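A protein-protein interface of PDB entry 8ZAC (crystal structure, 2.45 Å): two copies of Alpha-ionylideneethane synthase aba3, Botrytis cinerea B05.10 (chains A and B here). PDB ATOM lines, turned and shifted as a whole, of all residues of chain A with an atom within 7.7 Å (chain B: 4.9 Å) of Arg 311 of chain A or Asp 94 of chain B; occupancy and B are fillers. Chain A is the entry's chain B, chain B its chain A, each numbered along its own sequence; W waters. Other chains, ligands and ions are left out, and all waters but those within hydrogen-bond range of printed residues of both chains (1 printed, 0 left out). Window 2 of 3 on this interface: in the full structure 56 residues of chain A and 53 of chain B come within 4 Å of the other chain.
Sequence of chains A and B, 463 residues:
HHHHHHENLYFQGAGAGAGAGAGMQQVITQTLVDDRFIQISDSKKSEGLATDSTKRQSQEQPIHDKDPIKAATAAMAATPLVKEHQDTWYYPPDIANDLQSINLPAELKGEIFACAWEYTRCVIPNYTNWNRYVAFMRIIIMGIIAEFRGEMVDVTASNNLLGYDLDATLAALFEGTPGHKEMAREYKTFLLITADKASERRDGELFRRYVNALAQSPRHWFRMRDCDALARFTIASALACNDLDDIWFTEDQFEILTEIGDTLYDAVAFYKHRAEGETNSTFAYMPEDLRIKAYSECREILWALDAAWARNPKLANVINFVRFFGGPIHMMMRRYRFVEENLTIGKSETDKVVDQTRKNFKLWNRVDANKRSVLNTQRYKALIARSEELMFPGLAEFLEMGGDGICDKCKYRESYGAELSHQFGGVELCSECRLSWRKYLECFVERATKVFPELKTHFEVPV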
ATOM      1  N   ASP A 306     -14.739 -21.778 -14.017  1.00  0.00           N
ATOM      2  CA  ASP A 306     -14.116 -20.432 -13.865  1.00  0.00           C
ATOM      3  C   ASP A 306     -12.589 -20.578 -13.940  1.00  0.00           C
ATOM      4  O   ASP A 306     -11.976 -19.808 -14.671  1.00  0.00           O
ATOM      5  CB  ASP A 306     -14.578 -19.829 -12.526  1.00  0.00           C
ATOM      6  CG  ASP A 306     -14.342 -18.356 -12.305  1.00  0.00           C
ATOM      7  OD1 ASP A 306     -14.159 -17.605 -13.277  1.00  0.00           O
ATOM      8  OD2 ASP A 306     -14.397 -17.977 -11.148  1.00  0.00           O
ATOM      9  N   ALA A 307     -12.022 -21.502 -13.162  1.00  0.00           N
ATOM     10  CA  ALA A 307     -10.601 -21.934 -13.207  1.00  0.00           C
ATOM     11  C   ALA A 307     -10.195 -22.251 -14.652  1.00  0.00           C
ATOM     12  O   ALA A 307      -9.230 -21.639 -15.132  1.00  0.00           O
ATOM     13  CB  ALA A 307     -10.414 -23.134 -12.329  1.00  0.00           C
ATOM     14  N   ALA A 308     -10.952 -23.116 -15.342  1.00  0.00           N
ATOM     15  CA  ALA A 308     -10.639 -23.548 -16.726  1.00  0.00           C
ATOM     16  C   ALA A 308     -10.536 -22.320 -17.633  1.00  0.00           C
ATOM     17  O   ALA A 308      -9.614 -22.290 -18.487  1.00  0.00           O
ATOM     18  CB  ALA A 308     -11.660 -24.547 -17.228  1.00  0.00           C
ATOM     19  N   TRP A 309     -11.389 -21.311 -17.406  1.00  0.00           N
ATOM     20  CA  TRP A 309     -11.509 -20.096 -18.261  1.00  0.00           C
ATOM     21  C   TRP A 309     -10.550 -18.998 -17.780  1.00  0.00           C
ATOM     22  O   TRP A 309     -10.536 -17.882 -18.388  1.00  0.00           O
ATOM     23  CB  TRP A 309     -12.961 -19.605 -18.297  1.00  0.00           C
ATOM     24  CG  TRP A 309     -13.936 -20.568 -18.903  1.00  0.00           C
ATOM     25  CD1 TRP A 309     -13.660 -21.779 -19.466  1.00  0.00           C
ATOM     26  CD2 TRP A 309     -15.357 -20.365 -19.063  1.00  0.00           C
ATOM     27  NE1 TRP A 309     -14.808 -22.353 -19.943  1.00  0.00           N
ATOM     28  CE2 TRP A 309     -15.865 -21.510 -19.712  1.00  0.00           C
ATOM     29  CE3 TRP A 309     -16.247 -19.340 -18.715  1.00  0.00           C
ATOM     30  CZ2 TRP A 309     -17.221 -21.656 -20.006  1.00  0.00           C
ATOM     31  CZ3 TRP A 309     -17.584 -19.486 -19.008  1.00  0.00           C
ATOM     32  CH2 TRP A 309     -18.062 -20.632 -19.641  1.00  0.00           C
ATOM     33  N   ALA A 310      -9.742 -19.285 -16.759  1.00  0.00           N
ATOM     34  CA  ALA A 310      -8.716 -18.356 -16.234  1.00  0.00           C
ATOM     35  C   ALA A 310      -7.881 -17.765 -17.380  1.00  0.00           C
ATOM     36  O   ALA A 310      -7.620 -18.488 -18.384  1.00  0.00           O
ATOM     37  CB  ALA A 310      -7.870 -19.081 -15.221  1.00  0.00           C
ATOM     38  N   ARG A 311      -7.509 -16.486 -17.246  1.00  0.00           N
ATOM     39  CA  ARG A 311      -6.740 -15.677 -18.240  1.00  0.00           C
ATOM     40  C   ARG A 311      -7.651 -15.196 -19.378  1.00  0.00           C
ATOM     41  O   ARG A 311      -7.143 -14.439 -20.232  1.00  0.00           O
ATOM     42  CB  ARG A 311      -5.565 -16.452 -18.853  1.00  0.00           C
ATOM     43  CG  ARG A 311      -4.537 -16.989 -17.865  1.00  0.00           C
ATOM     44  CD  ARG A 311      -3.574 -17.974 -18.528  1.00  0.00           C
ATOM     45  NE  ARG A 311      -2.189 -17.834 -18.082  1.00  0.00           N
ATOM     46  CZ  ARG A 311      -1.392 -16.785 -18.336  1.00  0.00           C
ATOM     47  NH1 ARG A 311      -1.836 -15.747 -19.031  1.00  0.00           N
ATOM     48  NH2 ARG A 311      -0.149 -16.777 -17.883  1.00  0.00           N
ATOM     49  N   ASN A 312      -8.920 -15.626 -19.442  1.00  0.00           N
ATOM     50  CA  ASN A 312      -9.901 -15.077 -20.422  1.00  0.00           C
ATOM     51  C   ASN A 312     -10.885 -14.197 -19.656  1.00  0.00           C
ATOM     52  O   ASN A 312     -11.974 -14.634 -19.299  1.00  0.00           O
ATOM     53  CB  ASN A 312     -10.576 -16.171 -21.257  1.00  0.00           C
ATOM     54  CG  ASN A 312     -11.244 -15.658 -22.523  1.00  0.00           C
ATOM     55  OD1 ASN A 312     -11.302 -14.456 -22.789  1.00  0.00           O
ATOM     56  ND2 ASN A 312     -11.783 -16.571 -23.315  1.00  0.00           N
ATOM     57  N   PRO A 313     -10.540 -12.915 -19.389  1.00  0.00           N
ATOM     58  CA  PRO A 313     -11.412 -12.021 -18.624  1.00  0.00           C
ATOM     59  C   PRO A 313     -12.805 -11.861 -19.245  1.00  0.00           C
ATOM     60  O   PRO A 313     -13.719 -11.494 -18.541  1.00  0.00           O
ATOM     61  CB  PRO A 313     -10.663 -10.673 -18.664  1.00  0.00           C
ATOM     62  CG  PRO A 313      -9.803 -10.786 -19.906  1.00  0.00           C
ATOM     63  CD  PRO A 313      -9.332 -12.224 -19.864  1.00  0.00           C
ATOM     64  N   LYS A 314     -12.908 -12.104 -20.552  1.00  0.00           N
ATOM     65  CA  LYS A 314     -14.157 -11.973 -21.343  1.00  0.00           C
ATOM     66  C   LYS A 314     -15.198 -12.968 -20.814  1.00  0.00           C
ATOM     67  O   LYS A 314     -16.352 -12.574 -20.636  1.00  0.00           O
ATOM     68  CB  LYS A 314     -13.834 -12.180 -22.826  1.00  0.00           C
ATOM     69  CG  LYS A 314     -12.922 -11.109 -23.424  1.00  0.00           C
ATOM     70  CD  LYS A 314     -12.264 -11.473 -24.755  1.00  0.00           C
ATOM     71  CE  LYS A 314     -13.087 -11.102 -25.972  1.00  0.00           C
ATOM     72  NZ  LYS A 314     -12.299 -11.205 -27.222  1.00  0.00           N
ATOM     73  N   LEU A 315     -14.807 -14.219 -20.585  1.00  0.00           N
ATOM     74  CA  LEU A 315     -15.714 -15.290 -20.102  1.00  0.00           C
ATOM     75  C   LEU A 315     -16.031 -15.115 -18.609  1.00  0.00           C
ATOM     76  O   LEU A 315     -17.015 -15.716 -18.167  1.00  0.00           O
ATOM     77  CB  LEU A 315     -15.067 -16.651 -20.370  1.00  0.00           C
ATOM     78  CG  LEU A 315     -14.955 -17.050 -21.841  1.00  0.00           C
ATOM     79  CD1 LEU A 315     -14.406 -18.457 -21.969  1.00  0.00           C
ATOM     80  CD2 LEU A 315     -16.303 -16.944 -22.545  1.00  0.00           C
ATOM     81  N   PHE A 459      -5.126 -28.747 -14.278  1.00  0.00           N
ATOM     82  CA  PHE A 459      -3.729 -29.001 -13.830  1.00  0.00           C
ATOM     83  C   PHE A 459      -3.331 -27.952 -12.781  1.00  0.00           C
ATOM     84  O   PHE A 459      -2.889 -28.237 -11.663  1.00  0.00           O
ATOM     85  CB  PHE A 459      -2.769 -28.986 -15.025  1.00  0.00           C
ATOM     86  CG  PHE A 459      -1.437 -29.659 -14.789  1.00  0.00           C
ATOM     87  CD1 PHE A 459      -1.356 -31.036 -14.627  1.00  0.00           C
ATOM     88  CD2 PHE A 459      -0.260 -28.919 -14.739  1.00  0.00           C
ATOM     89  CE1 PHE A 459      -0.134 -31.657 -14.412  1.00  0.00           C
ATOM     90  CE2 PHE A 459       0.960 -29.542 -14.524  1.00  0.00           C
ATOM     91  CZ  PHE A 459       1.022 -30.909 -14.363  1.00  0.00           C
ATOM     92  N   PRO B  92      -6.236 -21.578 -10.869  1.00  0.00           N
ATOM     93  CA  PRO B  92      -5.474 -21.521 -12.107  1.00  0.00           C
ATOM     94  C   PRO B  92      -4.208 -22.382 -12.008  1.00  0.00           C
ATOM     95  O   PRO B  92      -3.759 -22.744 -10.916  1.00  0.00           O
ATOM     96  CB  PRO B  92      -5.124 -20.031 -12.255  1.00  0.00           C
ATOM     97  CG  PRO B  92      -5.912 -19.318 -11.180  1.00  0.00           C
ATOM     98  CD  PRO B  92      -6.163 -20.333 -10.094  1.00  0.00           C
ATOM     99  N   PRO B  93      -3.591 -22.772 -13.147  1.00  0.00           N
ATOM    100  CA  PRO B  93      -2.336 -23.511 -13.097  1.00  0.00           C
ATOM    101  C   PRO B  93      -1.238 -22.571 -12.569  1.00  0.00           C
ATOM    102  O   PRO B  93      -0.438 -23.017 -11.766  1.00  0.00           O
ATOM    103  CB  PRO B  93      -2.145 -23.981 -14.547  1.00  0.00           C
ATOM    104  CG  PRO B  93      -2.848 -22.924 -15.373  1.00  0.00           C
ATOM    105  CD  PRO B  93      -4.027 -22.490 -14.525  1.00  0.00           C
ATOM    106  N   ASP B  94      -1.278 -21.284 -12.950  1.00  0.00           N
ATOM    107  CA  ASP B  94      -0.228 -20.279 -12.633  1.00  0.00           C
ATOM    108  C   ASP B  94       0.350 -20.478 -11.232  1.00  0.00           C
ATOM    109  O   ASP B  94       1.570 -20.333 -11.091  1.00  0.00           O
ATOM    110  CB  ASP B  94      -0.778 -18.872 -12.741  1.00  0.00           C
ATOM    111  CG  ASP B  94      -1.136 -18.579 -14.172  1.00  0.00           C
ATOM    112  OD1 ASP B  94      -2.029 -19.301 -14.715  1.00  0.00           O
ATOM    113  OD2 ASP B  94      -0.484 -17.680 -14.745  1.00  0.00           O
ATOM    114  N   ILE B  95      -0.496 -20.765 -10.242  1.00  0.00           N
ATOM    115  CA  ILE B  95      -0.123 -20.858  -8.801  1.00  0.00           C
ATOM    116  C   ILE B  95      -0.145 -22.326  -8.406  1.00  0.00           C
ATOM    117  O   ILE B  95       0.050 -22.621  -7.215  1.00  0.00           O
ATOM    118  CB  ILE B  95      -1.087 -20.018  -7.935  1.00  0.00           C
ATOM    119  CG1 ILE B  95      -2.479 -20.652  -7.814  1.00  0.00           C
ATOM    120  CG2 ILE B  95      -1.172 -18.605  -8.486  1.00  0.00           C
ATOM    121  CD1 ILE B  95      -3.332 -20.051  -6.710  1.00  0.00           C
ATOM    122  N   ALA B  96      -0.403 -23.213  -9.365  1.00  0.00           N
ATOM    123  CA  ALA B  96      -0.640 -24.658  -9.124  1.00  0.00           C
ATOM    124  C   ALA B  96       0.623 -25.263  -8.509  1.00  0.00           C
ATOM    125  O   ALA B  96       0.495 -26.096  -7.589  1.00  0.00           O
ATOM    126  CB  ALA B  96      -1.042 -25.349 -10.409  1.00  0.00           C
ATOM    127  N   ASP B  98       2.994 -23.127  -7.189  1.00  0.00           N
ATOM    128  CA  ASP B  98       3.453 -22.251  -6.073  1.00  0.00           C
ATOM    129  C   ASP B  98       3.773 -23.191  -4.904  1.00  0.00           C
ATOM    130  O   ASP B  98       3.334 -24.358  -4.985  1.00  0.00           O
ATOM    131  CB  ASP B  98       2.415 -21.205  -5.635  1.00  0.00           C
ATOM    132  CG  ASP B  98       2.517 -19.818  -6.263  1.00  0.00           C
ATOM    133  OD1 ASP B  98       2.861 -19.713  -7.472  1.00  0.00           O
ATOM    134  OD2 ASP B  98       2.224 -18.831  -5.537  1.00  0.00           O
ATOM    135  N   TYR B 127     -10.859  -8.402 -14.418  1.00  0.00           N
ATOM    136  CA  TYR B 127      -9.417  -8.074 -14.600  1.00  0.00           C
ATOM    137  C   TYR B 127      -9.061  -7.821 -16.063  1.00  0.00           C
ATOM    138  O   TYR B 127      -9.795  -8.262 -16.960  1.00  0.00           O
ATOM    139  CB  TYR B 127      -8.521  -9.195 -14.091  1.00  0.00           C
ATOM    140  CG  TYR B 127      -8.673 -10.499 -14.822  1.00  0.00           C
ATOM    141  CD1 TYR B 127      -9.640 -11.409 -14.441  1.00  0.00           C
ATOM    142  CD2 TYR B 127      -7.830 -10.844 -15.866  1.00  0.00           C
ATOM    143  CE1 TYR B 127      -9.782 -12.624 -15.081  1.00  0.00           C
ATOM    144  CE2 TYR B 127      -7.960 -12.054 -16.522  1.00  0.00           C
ATOM    145  CZ  TYR B 127      -8.932 -12.953 -16.119  1.00  0.00           C
ATOM    146  OH  TYR B 127      -9.084 -14.159 -16.731  1.00  0.00           O
ATOM    147  N   TRP B 130      -3.406 -10.006 -15.940  1.00  0.00           N
ATOM    148  CA  TRP B 130      -3.346 -11.339 -15.294  1.00  0.00           C
ATOM    149  C   TRP B 130      -2.188 -11.425 -14.299  1.00  0.00           C
ATOM    150  O   TRP B 130      -2.374 -12.067 -13.249  1.00  0.00           O
ATOM    151  CB  TRP B 130      -3.260 -12.436 -16.342  1.00  0.00           C
ATOM    152  CG  TRP B 130      -3.137 -13.777 -15.704  1.00  0.00           C
ATOM    153  CD1 TRP B 130      -1.993 -14.495 -15.570  1.00  0.00           C
ATOM    154  CD2 TRP B 130      -4.174 -14.530 -15.037  1.00  0.00           C
ATOM    155  NE1 TRP B 130      -2.249 -15.651 -14.885  1.00  0.00           N
ATOM    156  CE2 TRP B 130      -3.576 -15.704 -14.548  1.00  0.00           C
ATOM    157  CE3 TRP B 130      -5.539 -14.333 -14.803  1.00  0.00           C
ATOM    158  CZ2 TRP B 130      -4.295 -16.690 -13.871  1.00  0.00           C
ATOM    159  CZ3 TRP B 130      -6.247 -15.297 -14.121  1.00  0.00           C
ATOM    160  CH2 TRP B 130      -5.634 -16.462 -13.670  1.00  0.00           C
ATOM    161  N   VAL B 134      -2.627 -12.570 -10.374  1.00  0.00           N
ATOM    162  CA  VAL B 134      -1.858 -13.698  -9.761  1.00  0.00           C
ATOM    163  C   VAL B 134      -1.048 -13.176  -8.560  1.00  0.00           C
ATOM    164  O   VAL B 134      -1.021 -13.861  -7.519  1.00  0.00           O
ATOM    165  CB  VAL B 134      -0.974 -14.402 -10.808  1.00  0.00           C
ATOM    166  CG1 VAL B 134      -0.072 -15.454 -10.185  1.00  0.00           C
ATOM    167  CG2 VAL B 134      -1.814 -15.026 -11.906  1.00  0.00           C
ATOM    168  N   ARG B 138      -1.288 -14.444  -4.692  1.00  0.00           N
ATOM    169  CA  ARG B 138      -0.090 -14.759  -3.853  1.00  0.00           C
ATOM    170  C   ARG B 138      -0.148 -13.933  -2.567  1.00  0.00           C
ATOM    171  O   ARG B 138       0.048 -14.495  -1.479  1.00  0.00           O
ATOM    172  CB  ARG B 138       1.193 -14.563  -4.667  1.00  0.00           C
ATOM    173  CG  ARG B 138       1.369 -15.639  -5.727  1.00  0.00           C
ATOM    174  CD  ARG B 138       2.604 -15.515  -6.589  1.00  0.00           C
ATOM    175  NE  ARG B 138       2.715 -16.688  -7.452  1.00  0.00           N
ATOM    176  CZ  ARG B 138       3.149 -16.650  -8.713  1.00  0.00           C
ATOM    177  NH1 ARG B 138       3.537 -15.510  -9.254  1.00  0.00           N
ATOM    178  NH2 ARG B 138       3.185 -17.750  -9.441  1.00  0.00           N
HETATM  179  O   HOH W   1     -11.578 -15.516 -16.322  1.00  0.00           O
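Among the printed residues, merely in contact across the chains: Arg 311 of chain A with Trp 130 of chain B, Phe 459 of chain A with Ala 96 of chain B, Ala 310 of chain A with Trp 130 of chain B and Ala 310 of chain A with Tyr 127 of chain B.
The backbone nitrogen (N) of Pro 313 of chain A sits close to the side-chain hydroxyl (OH) of Tyr 127 of chain B, 3.3 Å away.
OH of Tyr 127 of chain B sits at hydrogen-bond distance from N of Asn 312 of chain A (3.1 Å).
OH of Tyr 127 of chain B lies within hydrogen-bond range of N of Arg 311 of chain A (2.9 Å).
OD2 of Asp 94 of chain B lies within salt-bridge range of NH2 of Arg 311 of chain A (3.3 Å).
Water W1 lies within hydrogen-bond range of OH of Tyr 127 of chain B (2.9 Å), O of Asn 312 of chain A (3.1 Å) and O of Trp 309 of chain A (3.3 Å).
No position is printed for both chains.
Of the printed residues of chain B, Ala 310 of chain A touches Tyr 127 (3.9 Å) and Trp 130 (3.8 Å).
Of chain B, only Asp 94 (3.3 Å), Tyr 127 (2.9 Å) and Trp 130 (3.6 Å) come within 4 Å of Arg 311 of chain A.
Printed residues of chain B within 4 Å of Asn 312 of chain A: Tyr 127 (3.1 Å).
Lys 314 of chain A touches none of the printed residues of chain B.
No residue of chain A comes within 4 Å of Pro 93 of chain B.
Asp 94 of chain B touches just one residue of chain A: Arg 311.
Printed residues of chain A within 4 Å of Tyr 127 of chain B: Ala 310 (3.9 Å), Arg 311 (2.9 Å), Asn 312 (3.1 Å) and Pro 313 (3.1 Å).
Printed residues of chain A within 4 Å of Trp 130 of chain B: Ala 310 and Arg 311.
Val 134 of chain B touches none of the printed residues of chain A.
The nearest printed residue of chain A that does not touch Ala 96 of chain B is Ala 307 of chain A (9.8 Å).
The backbone carbonyl oxygen of Asp 94 of chain B sits at hydrogen-bond distance from the guanidinium group of Arg 138 of chain B.
The side-chain carboxylate of Asp 94 of chain B sits at hydrogen-bond distance from the indole nitrogen of Trp 130 of chain B.
Of the 10 printed residues of chain B, 4 touch a printed residue of chain A.
Of the 11 printed residues of chain A, 5 touch a printed residue of chain B.
Printed residues of chain A that touch a printed residue of chain B: Ala 310, Arg 311, Asn 312, Pro 313 and Phe 459.
Along chain A the printed residues that touch a printed residue of chain B span positions 310 to 459.
Among the printed residues, 8 pairs touch across the chains.
Among the printed residues, Asp or Glu carboxylates within 4 Å of a Lys or Arg side-chain nitrogen of the other chain: Arg 311 of chain A with Asp 94 of chain B (3.3 Å).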
